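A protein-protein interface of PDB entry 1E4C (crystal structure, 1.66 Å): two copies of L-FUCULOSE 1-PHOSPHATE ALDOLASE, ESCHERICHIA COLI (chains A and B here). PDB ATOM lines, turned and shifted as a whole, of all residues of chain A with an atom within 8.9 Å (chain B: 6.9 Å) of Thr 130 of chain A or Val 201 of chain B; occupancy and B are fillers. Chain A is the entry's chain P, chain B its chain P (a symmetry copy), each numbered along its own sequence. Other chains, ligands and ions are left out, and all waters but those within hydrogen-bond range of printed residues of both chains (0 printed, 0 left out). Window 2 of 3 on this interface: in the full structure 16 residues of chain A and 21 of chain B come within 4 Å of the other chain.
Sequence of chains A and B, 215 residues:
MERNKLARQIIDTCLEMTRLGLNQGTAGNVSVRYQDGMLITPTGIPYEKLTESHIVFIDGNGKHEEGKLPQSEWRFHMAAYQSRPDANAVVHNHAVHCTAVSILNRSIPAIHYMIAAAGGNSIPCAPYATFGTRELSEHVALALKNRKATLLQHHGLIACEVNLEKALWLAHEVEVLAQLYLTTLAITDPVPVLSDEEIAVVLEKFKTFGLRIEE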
ATOM      1  N   SER A  72       3.766  -7.230 -35.758  1.00  0.00           N
ATOM      2  CA  SER A  72       3.864  -6.975 -34.331  1.00  0.00           C
ATOM      3  C   SER A  72       3.641  -5.532 -33.918  1.00  0.00           C
ATOM      4  O   SER A  72       3.358  -5.315 -32.733  1.00  0.00           O
ATOM      5  CB  SER A  72       5.190  -7.517 -33.784  1.00  0.00           C
ATOM      6  OG  SER A  72       6.269  -6.724 -34.233  1.00  0.00           O
ATOM      7  N   GLU A  73       3.735  -4.560 -34.826  1.00  0.00           N
ATOM      8  CA  GLU A  73       3.466  -3.174 -34.476  1.00  0.00           C
ATOM      9  C   GLU A  73       2.139  -2.662 -35.018  1.00  0.00           C
ATOM     10  O   GLU A  73       1.895  -1.448 -35.052  1.00  0.00           O
ATOM     11  CB  GLU A  73       4.611  -2.298 -35.029  1.00  0.00           C
ATOM     12  CG  GLU A  73       5.868  -2.482 -34.173  1.00  0.00           C
ATOM     13  CD  GLU A  73       7.095  -1.945 -34.864  1.00  0.00           C
ATOM     14  OE1 GLU A  73       7.364  -2.315 -36.017  1.00  0.00           O
ATOM     15  OE2 GLU A  73       7.781  -1.128 -34.223  1.00  0.00           O
ATOM     16  N   ARG A  75      -0.817  -2.460 -33.711  1.00  0.00           N
ATOM     17  CA  ARG A  75      -1.620  -1.655 -32.799  1.00  0.00           C
ATOM     18  C   ARG A  75      -1.393  -0.158 -32.901  1.00  0.00           C
ATOM     19  O   ARG A  75      -2.385   0.587 -32.794  1.00  0.00           O
ATOM     20  CB  ARG A  75      -1.427  -2.148 -31.356  1.00  0.00           C
ATOM     21  CG  ARG A  75      -2.149  -3.474 -31.115  1.00  0.00           C
ATOM     22  CD  ARG A  75      -1.953  -3.891 -29.655  1.00  0.00           C
ATOM     23  NE  ARG A  75      -3.030  -4.810 -29.279  1.00  0.00           N
ATOM     24  CZ  ARG A  75      -2.990  -6.117 -29.512  1.00  0.00           C
ATOM     25  NH1 ARG A  75      -1.933  -6.662 -30.091  1.00  0.00           N
ATOM     26  NH2 ARG A  75      -4.009  -6.891 -29.160  1.00  0.00           N
ATOM     27  N   PHE A  76      -0.174   0.357 -33.111  1.00  0.00           N
ATOM     28  CA  PHE A  76      -0.023   1.812 -33.180  1.00  0.00           C
ATOM     29  C   PHE A  76      -0.446   2.369 -34.530  1.00  0.00           C
ATOM     30  O   PHE A  76      -0.706   3.569 -34.624  1.00  0.00           O
ATOM     31  CB  PHE A  76       1.321   2.295 -32.675  1.00  0.00           C
ATOM     32  CG  PHE A  76       2.603   1.941 -33.352  1.00  0.00           C
ATOM     33  CD1 PHE A  76       2.755   1.947 -34.722  1.00  0.00           C
ATOM     34  CD2 PHE A  76       3.709   1.620 -32.570  1.00  0.00           C
ATOM     35  CE1 PHE A  76       3.971   1.626 -35.316  1.00  0.00           C
ATOM     36  CE2 PHE A  76       4.925   1.301 -33.157  1.00  0.00           C
ATOM     37  CZ  PHE A  76       5.051   1.315 -34.524  1.00  0.00           C
ATOM     38  N   PRO A 127       6.741   9.173 -25.203  1.00  0.00           N
ATOM     39  CA  PRO A 127       7.495   8.363 -24.265  1.00  0.00           C
ATOM     40  C   PRO A 127       7.600   6.902 -24.639  1.00  0.00           C
ATOM     41  O   PRO A 127       6.687   6.315 -25.238  1.00  0.00           O
ATOM     42  CB  PRO A 127       6.745   8.514 -22.939  1.00  0.00           C
ATOM     43  CG  PRO A 127       5.721   9.553 -23.133  1.00  0.00           C
ATOM     44  CD  PRO A 127       5.597   9.882 -24.595  1.00  0.00           C
ATOM     45  N   TYR A 128       8.698   6.250 -24.254  1.00  0.00           N
ATOM     46  CA  TYR A 128       8.915   4.850 -24.510  1.00  0.00           C
ATOM     47  C   TYR A 128       7.907   3.917 -23.834  1.00  0.00           C
ATOM     48  O   TYR A 128       7.593   4.048 -22.644  1.00  0.00           O
ATOM     49  CB  TYR A 128      10.328   4.435 -23.990  1.00  0.00           C
ATOM     50  CG  TYR A 128      10.580   2.974 -24.345  1.00  0.00           C
ATOM     51  CD1 TYR A 128      10.989   2.580 -25.606  1.00  0.00           C
ATOM     52  CD2 TYR A 128      10.379   1.994 -23.382  1.00  0.00           C
ATOM     53  CE1 TYR A 128      11.172   1.250 -25.917  1.00  0.00           C
ATOM     54  CE2 TYR A 128      10.561   0.665 -23.682  1.00  0.00           C
ATOM     55  CZ  TYR A 128      10.961   0.288 -24.940  1.00  0.00           C
ATOM     56  OH  TYR A 128      11.141  -1.036 -25.235  1.00  0.00           O
ATOM     57  N   ALA A 129       7.468   2.912 -24.562  1.00  0.00           N
ATOM     58  CA  ALA A 129       6.718   1.771 -24.064  1.00  0.00           C
ATOM     59  C   ALA A 129       7.047   0.619 -25.014  1.00  0.00           C
ATOM     60  O   ALA A 129       7.375   0.866 -26.188  1.00  0.00           O
ATOM     61  CB  ALA A 129       5.232   1.994 -23.930  1.00  0.00           C
ATOM     62  N   THR A 130       7.024  -0.614 -24.540  1.00  0.00           N
ATOM     63  CA  THR A 130       7.366  -1.754 -25.378  1.00  0.00           C
ATOM     64  C   THR A 130       6.572  -1.786 -26.673  1.00  0.00           C
ATOM     65  O   THR A 130       5.370  -1.548 -26.642  1.00  0.00           O
ATOM     66  CB  THR A 130       7.140  -3.094 -24.635  1.00  0.00           C
ATOM     67  OG1 THR A 130       7.751  -3.006 -23.343  1.00  0.00           O
ATOM     68  CG2 THR A 130       7.753  -4.251 -25.393  1.00  0.00           C
ATOM     69  N   PHE A 131       7.222  -2.088 -27.795  1.00  0.00           N
ATOM     70  CA  PHE A 131       6.508  -2.222 -29.062  1.00  0.00           C
ATOM     71  C   PHE A 131       5.378  -3.246 -28.912  1.00  0.00           C
ATOM     72  O   PHE A 131       5.474  -4.218 -28.151  1.00  0.00           O
ATOM     73  CB  PHE A 131       7.423  -2.657 -30.205  1.00  0.00           C
ATOM     74  CG  PHE A 131       7.964  -4.061 -30.166  1.00  0.00           C
ATOM     75  CD1 PHE A 131       9.111  -4.361 -29.454  1.00  0.00           C
ATOM     76  CD2 PHE A 131       7.326  -5.085 -30.846  1.00  0.00           C
ATOM     77  CE1 PHE A 131       9.615  -5.646 -29.416  1.00  0.00           C
ATOM     78  CE2 PHE A 131       7.822  -6.376 -30.819  1.00  0.00           C
ATOM     79  CZ  PHE A 131       8.970  -6.660 -30.105  1.00  0.00           C
ATOM     80  N   GLY A 132       4.270  -2.987 -29.604  1.00  0.00           N
ATOM     81  CA  GLY A 132       3.120  -3.858 -29.605  1.00  0.00           C
ATOM     82  C   GLY A 132       2.195  -3.775 -28.411  1.00  0.00           C
ATOM     83  O   GLY A 132       1.278  -4.601 -28.280  1.00  0.00           O
ATOM     84  N   THR A 133       2.424  -2.828 -27.498  1.00  0.00           N
ATOM     85  CA  THR A 133       1.600  -2.718 -26.307  1.00  0.00           C
ATOM     86  C   THR A 133       0.531  -1.638 -26.451  1.00  0.00           C
ATOM     87  O   THR A 133       0.661  -0.681 -27.204  1.00  0.00           O
ATOM     88  CB  THR A 133       2.429  -2.409 -25.043  1.00  0.00           C
ATOM     89  OG1 THR A 133       3.129  -1.169 -25.190  1.00  0.00           O
ATOM     90  CG2 THR A 133       3.433  -3.521 -24.758  1.00  0.00           C
ATOM     91  N   ARG A 134      -0.516  -1.787 -25.639  1.00  0.00           N
ATOM     92  CA  ARG A 134      -1.594  -0.808 -25.569  1.00  0.00           C
ATOM     93  C   ARG A 134      -1.026   0.515 -25.059  1.00  0.00           C
ATOM     94  O   ARG A 134      -1.392   1.580 -25.535  1.00  0.00           O
ATOM     95  CB  ARG A 134      -2.700  -1.279 -24.619  1.00  0.00           C
ATOM     96  CG  ARG A 134      -4.078  -1.350 -25.266  1.00  0.00           C
ATOM     97  CD  ARG A 134      -4.092  -2.387 -26.387  1.00  0.00           C
ATOM     98  NE  ARG A 134      -5.313  -2.358 -27.188  1.00  0.00           N
ATOM     99  CZ  ARG A 134      -6.105  -3.408 -27.403  1.00  0.00           C
ATOM    100  NH1 ARG A 134      -5.824  -4.598 -26.888  1.00  0.00           N
ATOM    101  NH2 ARG A 134      -7.194  -3.249 -28.150  1.00  0.00           N
ATOM    102  N   GLU A 135      -0.113   0.434 -24.091  1.00  0.00           N
ATOM    103  CA  GLU A 135       0.548   1.612 -23.547  1.00  0.00           C
ATOM    104  C   GLU A 135       1.225   2.433 -24.641  1.00  0.00           C
ATOM    105  O   GLU A 135       1.046   3.647 -24.716  1.00  0.00           O
ATOM    106  CB  GLU A 135       1.556   1.150 -22.495  1.00  0.00           C
ATOM    107  CG  GLU A 135       2.053   2.242 -21.566  1.00  0.00           C
ATOM    108  CD  GLU A 135       3.093   1.710 -20.590  1.00  0.00           C
ATOM    109  OE1 GLU A 135       3.121   0.483 -20.331  1.00  0.00           O
ATOM    110  OE2 GLU A 135       3.899   2.512 -20.072  1.00  0.00           O
ATOM    111  N   LEU A 136       1.982   1.785 -25.527  1.00  0.00           N
ATOM    112  CA  LEU A 136       2.626   2.532 -26.619  1.00  0.00           C
ATOM    113  C   LEU A 136       1.566   3.153 -27.523  1.00  0.00           C
ATOM    114  O   LEU A 136       1.690   4.314 -27.923  1.00  0.00           O
ATOM    115  CB  LEU A 136       3.593   1.655 -27.407  1.00  0.00           C
ATOM    116  CG  LEU A 136       4.350   2.334 -28.555  1.00  0.00           C
ATOM    117  CD1 LEU A 136       5.143   3.536 -28.064  1.00  0.00           C
ATOM    118  CD2 LEU A 136       5.265   1.333 -29.258  1.00  0.00           C
ATOM    119  N   SER A 137       0.487   2.416 -27.815  1.00  0.00           N
ATOM    120  CA  SER A 137      -0.606   2.920 -28.626  1.00  0.00           C
ATOM    121  C   SER A 137      -1.201   4.207 -28.067  1.00  0.00           C
ATOM    122  O   SER A 137      -1.449   5.138 -28.839  1.00  0.00           O
ATOM    123  CB  SER A 137      -1.769   1.920 -28.744  1.00  0.00           C
ATOM    124  OG  SER A 137      -1.406   0.901 -29.643  1.00  0.00           O
ATOM    125  N   HIS A 139       0.248   6.451 -26.078  1.00  0.00           N
ATOM    126  CA  HIS A 139       1.190   7.567 -26.203  1.00  0.00           C
ATOM    127  C   HIS A 139       1.181   8.096 -27.641  1.00  0.00           C
ATOM    128  O   HIS A 139       1.258   9.307 -27.855  1.00  0.00           O
ATOM    129  CB  HIS A 139       2.615   7.180 -25.845  1.00  0.00           C
ATOM    130  CG  HIS A 139       2.825   6.862 -24.399  1.00  0.00           C
ATOM    131  ND1 HIS A 139       3.619   5.803 -24.003  1.00  0.00           N
ATOM    132  CD2 HIS A 139       2.364   7.445 -23.272  1.00  0.00           C
ATOM    133  CE1 HIS A 139       3.638   5.746 -22.684  1.00  0.00           C
ATOM    134  NE2 HIS A 139       2.893   6.726 -22.224  1.00  0.00           N
ATOM    135  N   LEU A 152       9.229   8.466 -31.535  1.00  0.00           N
ATOM    136  CA  LEU A 152       8.928   7.462 -30.511  1.00  0.00           C
ATOM    137  C   LEU A 152      10.217   7.233 -29.715  1.00  0.00           C
ATOM    138  O   LEU A 152      11.189   6.749 -30.304  1.00  0.00           O
ATOM    139  CB  LEU A 152       8.436   6.166 -31.157  1.00  0.00           C
ATOM    140  CG  LEU A 152       6.985   6.210 -31.667  1.00  0.00           C
ATOM    141  CD1 LEU A 152       6.924   6.831 -33.055  1.00  0.00           C
ATOM    142  CD2 LEU A 152       6.362   4.826 -31.669  1.00  0.00           C
ATOM    143  N   GLN A 153      10.277   7.643 -28.449  1.00  0.00           N
ATOM    144  CA  GLN A 153      11.509   7.542 -27.662  1.00  0.00           C
ATOM    145  C   GLN A 153      12.171   6.180 -27.724  1.00  0.00           C
ATOM    146  O   GLN A 153      11.488   5.167 -27.632  1.00  0.00           O
ATOM    147  CB  GLN A 153      11.181   7.869 -26.189  1.00  0.00           C
ATOM    148  CG  GLN A 153      12.426   8.062 -25.342  1.00  0.00           C
ATOM    149  CD  GLN A 153      12.157   8.126 -23.852  1.00  0.00           C
ATOM    150  OE1 GLN A 153      13.070   8.440 -23.063  1.00  0.00           O
ATOM    151  NE2 GLN A 153      10.939   7.854 -23.437  1.00  0.00           N
ATOM    152  N   HIS A 154      13.479   6.089 -27.960  1.00  0.00           N
ATOM    153  CA  HIS A 154      14.252   4.876 -28.109  1.00  0.00           C
ATOM    154  C   HIS A 154      13.696   3.967 -29.201  1.00  0.00           C
ATOM    155  O   HIS A 154      13.850   2.746 -29.096  1.00  0.00           O
ATOM    156  CB  HIS A 154      14.353   4.090 -26.790  1.00  0.00           C
ATOM    157  CG  HIS A 154      15.177   4.770 -25.741  1.00  0.00           C
ATOM    158  ND1 HIS A 154      16.548   4.916 -25.805  1.00  0.00           N
ATOM    159  CD2 HIS A 154      14.788   5.313 -24.558  1.00  0.00           C
ATOM    160  CE1 HIS A 154      16.960   5.551 -24.711  1.00  0.00           C
ATOM    161  NE2 HIS A 154      15.924   5.791 -23.929  1.00  0.00           N
ATOM    162  N   HIS A 155      13.101   4.554 -30.260  1.00  0.00           N
ATOM    163  CA  HIS A 155      12.463   3.661 -31.234  1.00  0.00           C
ATOM    164  C   HIS A 155      12.535   4.192 -32.651  1.00  0.00           C
ATOM    165  O   HIS A 155      13.210   3.562 -33.481  1.00  0.00           O
ATOM    166  CB  HIS A 155      11.011   3.425 -30.775  1.00  0.00           C
ATOM    167  CG  HIS A 155      10.285   2.392 -31.596  1.00  0.00           C
ATOM    168  ND1 HIS A 155       9.265   1.623 -31.084  1.00  0.00           N
ATOM    169  CD2 HIS A 155      10.433   2.005 -32.873  1.00  0.00           C
ATOM    170  CE1 HIS A 155       8.831   0.806 -32.044  1.00  0.00           C
ATOM    171  NE2 HIS A 155       9.532   1.018 -33.153  1.00  0.00           N
ATOM    172  N   ASP B 196      17.633  -2.753 -17.795  1.00  0.00           N
ATOM    173  CA  ASP B 196      17.766  -4.190 -18.015  1.00  0.00           C
ATOM    174  C   ASP B 196      16.422  -4.899 -17.983  1.00  0.00           C
ATOM    175  O   ASP B 196      16.180  -5.846 -18.737  1.00  0.00           O
ATOM    176  CB  ASP B 196      18.728  -4.800 -16.992  1.00  0.00           C
ATOM    177  CG  ASP B 196      20.169  -4.468 -17.304  1.00  0.00           C
ATOM    178  OD1 ASP B 196      20.489  -3.883 -18.363  1.00  0.00           O
ATOM    179  OD2 ASP B 196      21.048  -4.796 -16.479  1.00  0.00           O
ATOM    180  N   GLU B 197      15.486  -4.430 -17.167  1.00  0.00           N
ATOM    181  CA  GLU B 197      14.126  -4.921 -17.096  1.00  0.00           C
ATOM    182  C   GLU B 197      13.425  -4.815 -18.455  1.00  0.00           C
ATOM    183  O   GLU B 197      12.783  -5.763 -18.902  1.00  0.00           O
ATOM    184  CB  GLU B 197      13.273  -4.102 -16.118  1.00  0.00           C
ATOM    185  CG  GLU B 197      13.867  -3.914 -14.739  1.00  0.00           C
ATOM    186  CD  GLU B 197      14.944  -2.843 -14.667  1.00  0.00           C
ATOM    187  OE1 GLU B 197      14.568  -1.653 -14.520  1.00  0.00           O
ATOM    188  OE2 GLU B 197      16.153  -3.181 -14.742  1.00  0.00           O
ATOM    189  N   GLU B 198      13.569  -3.634 -19.076  1.00  0.00           N
ATOM    190  CA  GLU B 198      12.952  -3.417 -20.384  1.00  0.00           C
ATOM    191  C   GLU B 198      13.572  -4.288 -21.467  1.00  0.00           C
ATOM    192  O   GLU B 198      12.854  -4.865 -22.294  1.00  0.00           O
ATOM    193  CB  GLU B 198      13.014  -1.939 -20.789  1.00  0.00           C
ATOM    194  CG  GLU B 198      12.291  -1.661 -22.104  1.00  0.00           C
ATOM    195  CD  GLU B 198      10.869  -2.217 -22.125  1.00  0.00           C
ATOM    196  OE1 GLU B 198      10.212  -2.103 -21.060  1.00  0.00           O
ATOM    197  OE2 GLU B 198      10.439  -2.769 -23.163  1.00  0.00           O
ATOM    198  N   ILE B 199      14.902  -4.434 -21.462  1.00  0.00           N
ATOM    199  CA  ILE B 199      15.525  -5.323 -22.453  1.00  0.00           C
ATOM    200  C   ILE B 199      15.111  -6.769 -22.235  1.00  0.00           C
ATOM    201  O   ILE B 199      14.879  -7.514 -23.187  1.00  0.00           O
ATOM    202  CB  ILE B 199      17.052  -5.145 -22.458  1.00  0.00           C
ATOM    203  CG1 ILE B 199      17.419  -3.731 -22.937  1.00  0.00           C
ATOM    204  CG2 ILE B 199      17.739  -6.200 -23.318  1.00  0.00           C
ATOM    205  CD1 ILE B 199      16.900  -3.355 -24.315  1.00  0.00           C
ATOM    206  N   ALA B 200      14.920  -7.206 -20.990  1.00  0.00           N
ATOM    207  CA  ALA B 200      14.438  -8.564 -20.719  1.00  0.00           C
ATOM    208  C   ALA B 200      13.089  -8.829 -21.373  1.00  0.00           C
ATOM    209  O   ALA B 200      12.878  -9.878 -21.978  1.00  0.00           O
ATOM    210  CB  ALA B 200      14.382  -8.801 -19.213  1.00  0.00           C
ATOM    211  N   VAL B 201      12.173  -7.872 -21.321  1.00  0.00           N
ATOM    212  CA  VAL B 201      10.871  -7.980 -21.971  1.00  0.00           C
ATOM    213  C   VAL B 201      11.021  -8.110 -23.479  1.00  0.00           C
ATOM    214  O   VAL B 201      10.400  -8.933 -24.143  1.00  0.00           O
ATOM    215  CB  VAL B 201      10.027  -6.733 -21.642  1.00  0.00           C
ATOM    216  CG1 VAL B 201       8.745  -6.661 -22.452  1.00  0.00           C
ATOM    217  CG2 VAL B 201       9.691  -6.670 -20.157  1.00  0.00           C
ATOM    218  N   VAL B 202      11.896  -7.278 -24.064  1.00  0.00           N
ATOM    219  CA  VAL B 202      12.110  -7.318 -25.512  1.00  0.00           C
ATOM    220  C   VAL B 202      12.706  -8.639 -25.951  1.00  0.00           C
ATOM    221  O   VAL B 202      12.280  -9.256 -26.932  1.00  0.00           O
ATOM    222  CB  VAL B 202      13.001  -6.122 -25.919  1.00  0.00           C
ATOM    223  CG1 VAL B 202      13.359  -6.213 -27.400  1.00  0.00           C
ATOM    224  CG2 VAL B 202      12.288  -4.821 -25.574  1.00  0.00           C
ATOM    225  N   LEU B 203      13.700  -9.138 -25.205  1.00  0.00           N
ATOM    226  CA  LEU B 203      14.327 -10.420 -25.508  1.00  0.00           C
ATOM    227  C   LEU B 203      13.321 -11.567 -25.557  1.00  0.00           C
ATOM    228  O   LEU B 203      13.375 -12.426 -26.444  1.00  0.00           O
ATOM    229  CB  LEU B 203      15.369 -10.730 -24.431  1.00  0.00           C
ATOM    230  CG  LEU B 203      16.788 -10.239 -24.722  1.00  0.00           C
ATOM    231  CD1 LEU B 203      17.643 -10.464 -23.488  1.00  0.00           C
ATOM    232  CD2 LEU B 203      17.351 -10.951 -25.946  1.00  0.00           C
ATOM    233  N   GLU B 204      12.388 -11.585 -24.610  1.00  0.00           N
ATOM    234  CA  GLU B 204      11.344 -12.612 -24.609  1.00  0.00           C
ATOM    235  C   GLU B 204      10.490 -12.473 -25.862  1.00  0.00           C
ATOM    236  O   GLU B 204      10.288 -13.452 -26.589  1.00  0.00           O
ATOM    237  CB  GLU B 204      10.488 -12.526 -23.348  1.00  0.00           C
ATOM    238  CG  GLU B 204       9.599 -13.745 -23.122  1.00  0.00           C
ATOM    239  CD  GLU B 204      10.312 -14.840 -22.344  1.00  0.00           C
ATOM    240  OE1 GLU B 204      11.231 -15.493 -22.898  1.00  0.00           O
ATOM    241  OE2 GLU B 204       9.963 -15.047 -21.154  1.00  0.00           O
ATOM    242  N   LYS B 205      10.045 -11.256 -26.183  1.00  0.00           N
ATOM    243  CA  LYS B 205       9.242 -11.027 -27.380  1.00  0.00           C
ATOM    244  C   LYS B 205       9.911 -11.455 -28.674  1.00  0.00           C
ATOM    245  O   LYS B 205       9.236 -11.963 -29.579  1.00  0.00           O
ATOM    246  CB  LYS B 205       8.857  -9.544 -27.475  1.00  0.00           C
ATOM    247  CG  LYS B 205       7.786  -9.128 -26.483  1.00  0.00           C
ATOM    248  CD  LYS B 205       7.011  -7.921 -26.991  1.00  0.00           C
ATOM    249  CE  LYS B 205       5.519  -8.041 -26.709  1.00  0.00           C
ATOM    250  NZ  LYS B 205       4.739  -6.909 -27.285  1.00  0.00           N
ATOM    251  N   PHE B 206      11.210 -11.233 -28.832  1.00  0.00           N
ATOM    252  CA  PHE B 206      11.948 -11.584 -30.036  1.00  0.00           C
ATOM    253  C   PHE B 206      12.023 -13.077 -30.324  1.00  0.00           C
ATOM    254  O   PHE B 206      11.917 -13.893 -29.378  1.00  0.00           O
ATOM    255  CB  PHE B 206      13.372 -11.012 -29.958  1.00  0.00           C
ATOM    256  CG  PHE B 206      13.518  -9.564 -30.336  1.00  0.00           C
ATOM    257  CD1 PHE B 206      12.447  -8.777 -30.714  1.00  0.00           C
ATOM    258  CD2 PHE B 206      14.778  -8.987 -30.322  1.00  0.00           C
ATOM    259  CE1 PHE B 206      12.608  -7.450 -31.063  1.00  0.00           C
ATOM    260  CE2 PHE B 206      14.959  -7.665 -30.668  1.00  0.00           C
ATOM    261  CZ  PHE B 206      13.872  -6.896 -31.033  1.00  0.00           C
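The side-chain hydroxyl (OH) of Tyr 128 of chain A lies within hydrogen-bond range of the side-chain carboxylate (OE2) of Glu 198 of chain B.
The side-chain hydroxyl (OG1) of Thr 130 of chain A lies within hydrogen-bond range of the side-chain carboxylate (OE2) of Glu 198 of chain B (2.7 Å).
The side-chain amino group (NZ) of Lys 205 of chain B sits at hydrogen-bond distance from the backbone carbonyl oxygen (O) of Phe 131 of chain A, at 2.9 Å.
No position is printed for both chains.
Printed residues of chain B that touch a printed residue of chain A: Glu 198, Val 201, Val 202, Lys 205 and Phe 206.
Hydrophobic or aromatic side chains of chain B within 4 Å of the printed part of chain A: Val 201, Val 202 and Phe 206.
Of chain B, only Glu 198 (2.7 Å) and Val 201 (3.9 Å) come within 4 Å of Thr 130 of chain A.
Of chain A, only Thr 130 (3.9 Å) comes within 4 Å of Val 201 of chain B.
Printed residues of chain B within 4 Å of Tyr 128 of chain A: Glu 198 and Val 202.
Printed residues of chain A within 4 Å of Val 202 of chain B: Tyr 128 (3.97 Å).
Arg 134 of chain A touches none of the printed residues of chain B.
N of Tyr 128 of chain A sits close to NE2 of Gln 153 of chain A, 2.9 Å away.
The backbone carbonyl oxygen of Thr 130 of chain A is in hydrogen-bond range of the side-chain hydroxyl of Thr 133 of chain A (2.7 Å).
Tyr 128 of chain A touches Val 202 of chain B (OH to CG2, 3.97 Å).
OG1 of Thr 130 of chain A touches CG1 of Val 201 of chain B, 3.9 Å away.
Phe 206 of chain B touches Phe 131 of chain A.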
